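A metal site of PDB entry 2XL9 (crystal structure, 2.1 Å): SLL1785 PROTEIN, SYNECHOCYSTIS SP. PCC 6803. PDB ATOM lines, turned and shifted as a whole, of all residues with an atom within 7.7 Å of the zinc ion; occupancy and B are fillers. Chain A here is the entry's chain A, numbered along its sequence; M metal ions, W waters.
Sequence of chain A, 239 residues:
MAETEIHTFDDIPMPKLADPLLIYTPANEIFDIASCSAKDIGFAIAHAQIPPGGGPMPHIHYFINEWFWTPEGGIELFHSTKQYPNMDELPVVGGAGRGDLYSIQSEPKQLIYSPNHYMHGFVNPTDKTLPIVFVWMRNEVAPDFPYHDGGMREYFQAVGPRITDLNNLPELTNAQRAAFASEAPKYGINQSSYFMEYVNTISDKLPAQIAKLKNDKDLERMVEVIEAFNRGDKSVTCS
Of the 21 residues printed, 4 come within 4 Å of the zinc ion.
Along chain A the residues within 4 Å of the zinc ion span positions 59 to 120.
The nearest printed residue that does not touch the zinc ion is Trp 136 (4.5 Å).
A ring nitrogen (ND1) of His 120 sits at hydrogen-bond distance from the side-chain hydroxyl of Ser 114 (2.7 Å).
NE1 of Trp 136 sits close to OE2 of Glu 66, at 3.2 Å.
N of Ser 114 lies within hydrogen-bond range of O of Glu 66, at 2.7 Å.
The side-chain amide oxygen of Gln 191 lies close to a ring nitrogen (ND1) of His 59.
The backbone carbonyl oxygen of Met 57 is in hydrogen-bond range of a ring nitrogen (ND1) of His 59.
Water W1 bridges the indole nitrogen (NE1) of Trp 136 (3.2 Å) and the side-chain carboxylate (OE2) of Glu 66 (3.4 Å).
The zinc ion is bound by water W1, 2.1 Å away.
NE2 of His 120 binds the zinc ion (2.2 Å).
A ring nitrogen (NE2) of His 61 is bound to the zinc ion, at 2.2 Å.
OE1 of Glu 66 binds the zinc ion (2.2 Å).
A ring nitrogen (NE2) of His 59 is bound to the zinc ion (2.2 Å).
Water W2 binds the zinc ion (2.6 Å).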
ATOM      1  N   PRO A  56     -11.889 -30.666 -15.943  1.00  0.00           N
ATOM      2  CA  PRO A  56     -11.261 -31.620 -16.866  1.00  0.00           C
ATOM      3  C   PRO A  56     -10.004 -32.240 -16.290  1.00  0.00           C
ATOM      4  O   PRO A  56      -9.282 -31.571 -15.542  1.00  0.00           O
ATOM      5  CB  PRO A  56     -10.858 -30.738 -18.053  1.00  0.00           C
ATOM      6  CG  PRO A  56     -10.619 -29.383 -17.448  1.00  0.00           C
ATOM      7  CD  PRO A  56     -11.613 -29.271 -16.334  1.00  0.00           C
ATOM      8  N   MET A  57      -9.750 -33.495 -16.668  1.00  0.00           N
ATOM      9  CA  MET A  57      -8.493 -34.193 -16.393  1.00  0.00           C
ATOM     10  C   MET A  57      -7.358 -33.485 -17.135  1.00  0.00           C
ATOM     11  O   MET A  57      -7.619 -32.813 -18.127  1.00  0.00           O
ATOM     12  CB  MET A  57      -8.587 -35.653 -16.848  1.00  0.00           C
ATOM     13  CG  MET A  57      -9.733 -36.528 -16.211  1.00  0.00           C
ATOM     14  SD  MET A  57      -9.612 -36.633 -14.278  1.00  0.00           S
ATOM     15  CE  MET A  57     -10.604 -35.028 -13.729  1.00  0.00           C
ATOM     16  N   PRO A  58      -6.093 -33.626 -16.661  1.00  0.00           N
ATOM     17  CA  PRO A  58      -4.992 -32.958 -17.366  1.00  0.00           C
ATOM     18  C   PRO A  58      -5.021 -33.185 -18.885  1.00  0.00           C
ATOM     19  O   PRO A  58      -5.305 -34.275 -19.361  1.00  0.00           O
ATOM     20  CB  PRO A  58      -3.735 -33.557 -16.728  1.00  0.00           C
ATOM     21  CG  PRO A  58      -4.168 -33.883 -15.319  1.00  0.00           C
ATOM     22  CD  PRO A  58      -5.620 -34.326 -15.449  1.00  0.00           C
ATOM     23  N   HIS A  59      -4.764 -32.106 -19.636  1.00  0.00           N
ATOM     24  CA  HIS A  59      -4.759 -32.166 -21.099  1.00  0.00           C
ATOM     25  C   HIS A  59      -3.833 -31.119 -21.703  1.00  0.00           C
ATOM     26  O   HIS A  59      -3.384 -30.176 -21.013  1.00  0.00           O
ATOM     27  CB  HIS A  59      -6.200 -32.039 -21.650  1.00  0.00           C
ATOM     28  CG  HIS A  59      -6.859 -30.746 -21.291  1.00  0.00           C
ATOM     29  ND1 HIS A  59      -7.498 -30.534 -20.086  1.00  0.00           N
ATOM     30  CD2 HIS A  59      -6.980 -29.582 -21.982  1.00  0.00           C
ATOM     31  CE1 HIS A  59      -7.978 -29.305 -20.042  1.00  0.00           C
ATOM     32  NE2 HIS A  59      -7.675 -28.704 -21.183  1.00  0.00           N
ATOM     33  N   ILE A  60      -3.575 -31.280 -23.011  1.00  0.00           N
ATOM     34  CA  ILE A  60      -2.685 -30.387 -23.760  1.00  0.00           C
ATOM     35  C   ILE A  60      -3.334 -29.935 -25.052  1.00  0.00           C
ATOM     36  O   ILE A  60      -3.839 -30.774 -25.796  1.00  0.00           O
ATOM     37  CB  ILE A  60      -1.361 -31.115 -24.138  1.00  0.00           C
ATOM     38  CG1 ILE A  60      -0.683 -31.722 -22.901  1.00  0.00           C
ATOM     39  CG2 ILE A  60      -0.452 -30.163 -24.888  1.00  0.00           C
ATOM     40  CD1 ILE A  60       0.312 -32.835 -23.230  1.00  0.00           C
ATOM     41  N   HIS A  61      -3.278 -28.627 -25.344  1.00  0.00           N
ATOM     42  CA  HIS A  61      -3.800 -28.063 -26.611  1.00  0.00           C
ATOM     43  C   HIS A  61      -2.772 -27.857 -27.713  1.00  0.00           C
ATOM     44  O   HIS A  61      -1.619 -27.512 -27.443  1.00  0.00           O
ATOM     45  CB  HIS A  61      -4.462 -26.722 -26.368  1.00  0.00           C
ATOM     46  CG  HIS A  61      -5.643 -26.804 -25.455  1.00  0.00           C
ATOM     47  ND1 HIS A  61      -6.916 -27.024 -25.898  1.00  0.00           N
ATOM     48  CD2 HIS A  61      -5.725 -26.736 -24.102  1.00  0.00           C
ATOM     49  CE1 HIS A  61      -7.753 -27.057 -24.870  1.00  0.00           C
ATOM     50  NE2 HIS A  61      -7.051 -26.889 -23.772  1.00  0.00           N
ATOM     51  N   ILE A  64      -5.169 -24.031 -29.963  1.00  0.00           N
ATOM     52  CA  ILE A  64      -5.487 -22.806 -29.207  1.00  0.00           C
ATOM     53  C   ILE A  64      -4.516 -22.457 -28.077  1.00  0.00           C
ATOM     54  O   ILE A  64      -3.814 -23.334 -27.535  1.00  0.00           O
ATOM     55  CB  ILE A  64      -6.961 -22.838 -28.621  1.00  0.00           C
ATOM     56  CG1 ILE A  64      -7.170 -23.997 -27.612  1.00  0.00           C
ATOM     57  CG2 ILE A  64      -7.993 -22.929 -29.745  1.00  0.00           C
ATOM     58  CD1 ILE A  64      -6.820 -23.656 -26.196  1.00  0.00           C
ATOM     59  N   GLU A  66      -4.945 -20.513 -24.264  1.00  0.00           N
ATOM     60  CA  GLU A  66      -6.066 -20.465 -23.329  1.00  0.00           C
ATOM     61  C   GLU A  66      -5.794 -19.515 -22.160  1.00  0.00           C
ATOM     62  O   GLU A  66      -4.684 -19.469 -21.622  1.00  0.00           O
ATOM     63  CB  GLU A  66      -6.382 -21.875 -22.788  1.00  0.00           C
ATOM     64  CG  GLU A  66      -7.611 -21.955 -21.885  1.00  0.00           C
ATOM     65  CD  GLU A  66      -8.053 -23.388 -21.545  1.00  0.00           C
ATOM     66  OE1 GLU A  66      -7.530 -24.364 -22.132  1.00  0.00           O
ATOM     67  OE2 GLU A  66      -8.955 -23.527 -20.692  1.00  0.00           O
ATOM     68  N   PHE A  68      -7.630 -18.610 -18.369  1.00  0.00           N
ATOM     69  CA  PHE A  68      -8.555 -18.943 -17.294  1.00  0.00           C
ATOM     70  C   PHE A  68      -8.778 -17.688 -16.437  1.00  0.00           C
ATOM     71  O   PHE A  68      -7.798 -17.049 -16.061  1.00  0.00           O
ATOM     72  CB  PHE A  68      -7.971 -20.010 -16.375  1.00  0.00           C
ATOM     73  CG  PHE A  68      -7.607 -21.307 -17.059  1.00  0.00           C
ATOM     74  CD1 PHE A  68      -8.532 -22.352 -17.148  1.00  0.00           C
ATOM     75  CD2 PHE A  68      -6.321 -21.501 -17.552  1.00  0.00           C
ATOM     76  CE1 PHE A  68      -8.178 -23.582 -17.758  1.00  0.00           C
ATOM     77  CE2 PHE A  68      -5.965 -22.715 -18.167  1.00  0.00           C
ATOM     78  CZ  PHE A  68      -6.887 -23.752 -18.251  1.00  0.00           C
ATOM     79  N   SER A 114      -2.268 -19.786 -20.457  1.00  0.00           N
ATOM     80  CA  SER A 114      -1.678 -21.086 -20.766  1.00  0.00           C
ATOM     81  C   SER A 114      -1.577 -21.289 -22.267  1.00  0.00           C
ATOM     82  O   SER A 114      -2.559 -21.700 -22.898  1.00  0.00           O
ATOM     83  CB  SER A 114      -2.500 -22.224 -20.133  1.00  0.00           C
ATOM     84  OG  SER A 114      -1.832 -23.492 -20.300  1.00  0.00           O
ATOM     85  N   TYR A 118       1.415 -26.684 -23.316  1.00  0.00           N
ATOM     86  CA  TYR A 118       1.547 -26.900 -21.876  1.00  0.00           C
ATOM     87  C   TYR A 118       0.466 -27.844 -21.377  1.00  0.00           C
ATOM     88  O   TYR A 118      -0.678 -27.785 -21.844  1.00  0.00           O
ATOM     89  CB  TYR A 118       1.436 -25.562 -21.124  1.00  0.00           C
ATOM     90  CG  TYR A 118       2.706 -24.745 -21.114  1.00  0.00           C
ATOM     91  CD1 TYR A 118       3.715 -25.005 -20.194  1.00  0.00           C
ATOM     92  CD2 TYR A 118       2.881 -23.681 -22.029  1.00  0.00           C
ATOM     93  CE1 TYR A 118       4.889 -24.240 -20.148  1.00  0.00           C
ATOM     94  CE2 TYR A 118       4.065 -22.902 -22.009  1.00  0.00           C
ATOM     95  CZ  TYR A 118       5.065 -23.185 -21.053  1.00  0.00           C
ATOM     96  OH  TYR A 118       6.223 -22.451 -20.992  1.00  0.00           O
ATOM     97  N   MET A 119       0.816 -28.724 -20.456  1.00  0.00           N
ATOM     98  CA  MET A 119      -0.192 -29.543 -19.794  1.00  0.00           C
ATOM     99  C   MET A 119      -0.901 -28.733 -18.702  1.00  0.00           C
ATOM    100  O   MET A 119      -0.236 -28.130 -17.852  1.00  0.00           O
ATOM    101  CB  MET A 119       0.451 -30.792 -19.212  1.00  0.00           C
ATOM    102  CG  MET A 119      -0.562 -31.814 -18.787  1.00  0.00           C
ATOM    103  SD  MET A 119       0.223 -33.291 -17.816  1.00  0.00           S
ATOM    104  CE  MET A 119       1.515 -33.937 -19.120  1.00  0.00           C
ATOM    105  N   HIS A 120      -2.236 -28.751 -18.709  1.00  0.00           N
ATOM    106  CA  HIS A 120      -3.008 -28.095 -17.676  1.00  0.00           C
ATOM    107  C   HIS A 120      -4.350 -28.785 -17.409  1.00  0.00           C
ATOM    108  O   HIS A 120      -4.760 -29.715 -18.103  1.00  0.00           O
ATOM    109  CB  HIS A 120      -3.207 -26.584 -17.976  1.00  0.00           C
ATOM    110  CG  HIS A 120      -4.130 -26.296 -19.123  1.00  0.00           C
ATOM    111  ND1 HIS A 120      -3.882 -25.292 -20.033  1.00  0.00           N
ATOM    112  CD2 HIS A 120      -5.292 -26.887 -19.515  1.00  0.00           C
ATOM    113  CE1 HIS A 120      -4.847 -25.274 -20.952  1.00  0.00           C
ATOM    114  NE2 HIS A 120      -5.716 -26.215 -20.647  1.00  0.00           N
ATOM    115  N   GLY A 121      -5.037 -28.303 -16.382  1.00  0.00           N
ATOM    116  CA  GLY A 121      -6.297 -28.859 -15.901  1.00  0.00           C
ATOM    117  C   GLY A 121      -6.699 -28.061 -14.680  1.00  0.00           C
ATOM    118  O   GLY A 121      -5.963 -27.162 -14.252  1.00  0.00           O
ATOM    119  N   PHE A 122      -7.868 -28.364 -14.130  1.00  0.00           N
ATOM    120  CA  PHE A 122      -8.321 -27.719 -12.906  1.00  0.00           C
ATOM    121  C   PHE A 122      -9.402 -28.540 -12.236  1.00  0.00           C
ATOM    122  O   PHE A 122     -10.046 -29.375 -12.873  1.00  0.00           O
ATOM    123  CB  PHE A 122      -8.839 -26.275 -13.149  1.00  0.00           C
ATOM    124  CG  PHE A 122     -10.188 -26.222 -13.846  1.00  0.00           C
ATOM    125  CD1 PHE A 122     -10.261 -26.081 -15.218  1.00  0.00           C
ATOM    126  CD2 PHE A 122     -11.369 -26.326 -13.115  1.00  0.00           C
ATOM    127  CE1 PHE A 122     -11.496 -26.060 -15.866  1.00  0.00           C
ATOM    128  CE2 PHE A 122     -12.610 -26.296 -13.736  1.00  0.00           C
ATOM    129  CZ  PHE A 122     -12.674 -26.156 -15.129  1.00  0.00           C
ATOM    130  N   PHE A 134     -13.455 -19.229 -19.513  1.00  0.00           N
ATOM    131  CA  PHE A 134     -12.393 -19.720 -20.384  1.00  0.00           C
ATOM    132  C   PHE A 134     -12.427 -18.938 -21.687  1.00  0.00           C
ATOM    133  O   PHE A 134     -13.509 -18.657 -22.240  1.00  0.00           O
ATOM    134  CB  PHE A 134     -12.615 -21.181 -20.766  1.00  0.00           C
ATOM    135  CG  PHE A 134     -12.841 -22.076 -19.607  1.00  0.00           C
ATOM    136  CD1 PHE A 134     -14.139 -22.464 -19.260  1.00  0.00           C
ATOM    137  CD2 PHE A 134     -11.767 -22.550 -18.860  1.00  0.00           C
ATOM    138  CE1 PHE A 134     -14.352 -23.294 -18.196  1.00  0.00           C
ATOM    139  CE2 PHE A 134     -11.980 -23.393 -17.762  1.00  0.00           C
ATOM    140  CZ  PHE A 134     -13.277 -23.777 -17.438  1.00  0.00           C
ATOM    141  N   TRP A 136     -10.636 -19.423 -25.472  1.00  0.00           N
ATOM    142  CA  TRP A 136      -9.791 -20.271 -26.287  1.00  0.00           C
ATOM    143  C   TRP A 136      -9.539 -19.615 -27.633  1.00  0.00           C
ATOM    144  O   TRP A 136     -10.402 -19.647 -28.507  1.00  0.00           O
ATOM    145  CB  TRP A 136     -10.423 -21.638 -26.496  1.00  0.00           C
ATOM    146  CG  TRP A 136     -10.766 -22.421 -25.247  1.00  0.00           C
ATOM    147  CD1 TRP A 136      -9.924 -23.190 -24.484  1.00  0.00           C
ATOM    148  CD2 TRP A 136     -12.068 -22.553 -24.676  1.00  0.00           C
ATOM    149  NE1 TRP A 136     -10.636 -23.785 -23.459  1.00  0.00           N
ATOM    150  CE2 TRP A 136     -11.948 -23.399 -23.547  1.00  0.00           C
ATOM    151  CE3 TRP A 136     -13.326 -22.028 -24.999  1.00  0.00           C
ATOM    152  CZ2 TRP A 136     -13.033 -23.739 -22.746  1.00  0.00           C
ATOM    153  CZ3 TRP A 136     -14.416 -22.367 -24.214  1.00  0.00           C
ATOM    154  CH2 TRP A 136     -14.261 -23.207 -23.095  1.00  0.00           C
ATOM    155  N   MET A 152     -12.715 -25.248 -30.310  1.00  0.00           N
ATOM    156  CA  MET A 152     -13.120 -25.625 -28.954  1.00  0.00           C
ATOM    157  C   MET A 152     -14.624 -25.633 -28.756  1.00  0.00           C
ATOM    158  O   MET A 152     -15.163 -26.531 -28.109  1.00  0.00           O
ATOM    159  CB  MET A 152     -12.452 -24.772 -27.877  1.00  0.00           C
ATOM    160  CG  MET A 152     -10.935 -24.995 -27.734  1.00  0.00           C
ATOM    161  SD  MET A 152     -10.438 -26.864 -27.418  1.00  0.00           S
ATOM    162  CE  MET A 152     -11.382 -27.032 -25.688  1.00  0.00           C
ATOM    163  N   PHE A 156     -16.893 -29.021 -27.585  1.00  0.00           N
ATOM    164  CA  PHE A 156     -17.888 -29.129 -26.511  1.00  0.00           C
ATOM    165  C   PHE A 156     -19.292 -29.409 -27.029  1.00  0.00           C
ATOM    166  O   PHE A 156     -20.061 -30.133 -26.382  1.00  0.00           O
ATOM    167  CB  PHE A 156     -17.862 -27.907 -25.607  1.00  0.00           C
ATOM    168  CG  PHE A 156     -16.607 -27.818 -24.765  1.00  0.00           C
ATOM    169  CD1 PHE A 156     -16.337 -28.770 -23.789  1.00  0.00           C
ATOM    170  CD2 PHE A 156     -15.709 -26.772 -24.963  1.00  0.00           C
ATOM    171  CE1 PHE A 156     -15.161 -28.694 -23.027  1.00  0.00           C
ATOM    172  CE2 PHE A 156     -14.534 -26.675 -24.193  1.00  0.00           C
ATOM    173  CZ  PHE A 156     -14.247 -27.634 -23.235  1.00  0.00           C
ATOM    174  N   ILE A 189      -6.597 -31.575 -29.176  1.00  0.00           N
ATOM    175  CA  ILE A 189      -6.415 -31.759 -27.736  1.00  0.00           C
ATOM    176  C   ILE A 189      -5.941 -33.170 -27.460  1.00  0.00           C
ATOM    177  O   ILE A 189      -6.535 -34.116 -27.957  1.00  0.00           O
ATOM    178  CB  ILE A 189      -7.734 -31.584 -26.915  1.00  0.00           C
ATOM    179  CG1 ILE A 189      -8.498 -30.314 -27.316  1.00  0.00           C
ATOM    180  CG2 ILE A 189      -7.445 -31.553 -25.382  1.00  0.00           C
ATOM    181  CD1 ILE A 189      -9.985 -30.381 -27.049  1.00  0.00           C
ATOM    182  N   GLN A 191      -6.327 -35.329 -24.416  1.00  0.00           N
ATOM    183  CA  GLN A 191      -7.090 -35.322 -23.165  1.00  0.00           C
ATOM    184  C   GLN A 191      -6.959 -36.672 -22.425  1.00  0.00           C
ATOM    185  O   GLN A 191      -7.428 -37.705 -22.928  1.00  0.00           O
ATOM    186  CB  GLN A 191      -8.578 -35.002 -23.472  1.00  0.00           C
ATOM    187  CG  GLN A 191      -9.550 -35.145 -22.274  1.00  0.00           C
ATOM    188  CD  GLN A 191      -9.238 -34.123 -21.191  1.00  0.00           C
ATOM    189  OE1 GLN A 191      -9.322 -32.930 -21.426  1.00  0.00           O
ATOM    190  NE2 GLN A 191      -8.850 -34.598 -20.005  1.00  0.00           N
HETATM  191 ZN    ZN M   1      -7.585 -26.531 -21.689  1.00  0.00          ZN
HETATM  192  O   HOH W   1      -9.672 -26.507 -22.200  1.00  0.00           O
HETATM  193  O   HOH W   2      -9.409 -25.732 -20.029  1.00  0.00           O
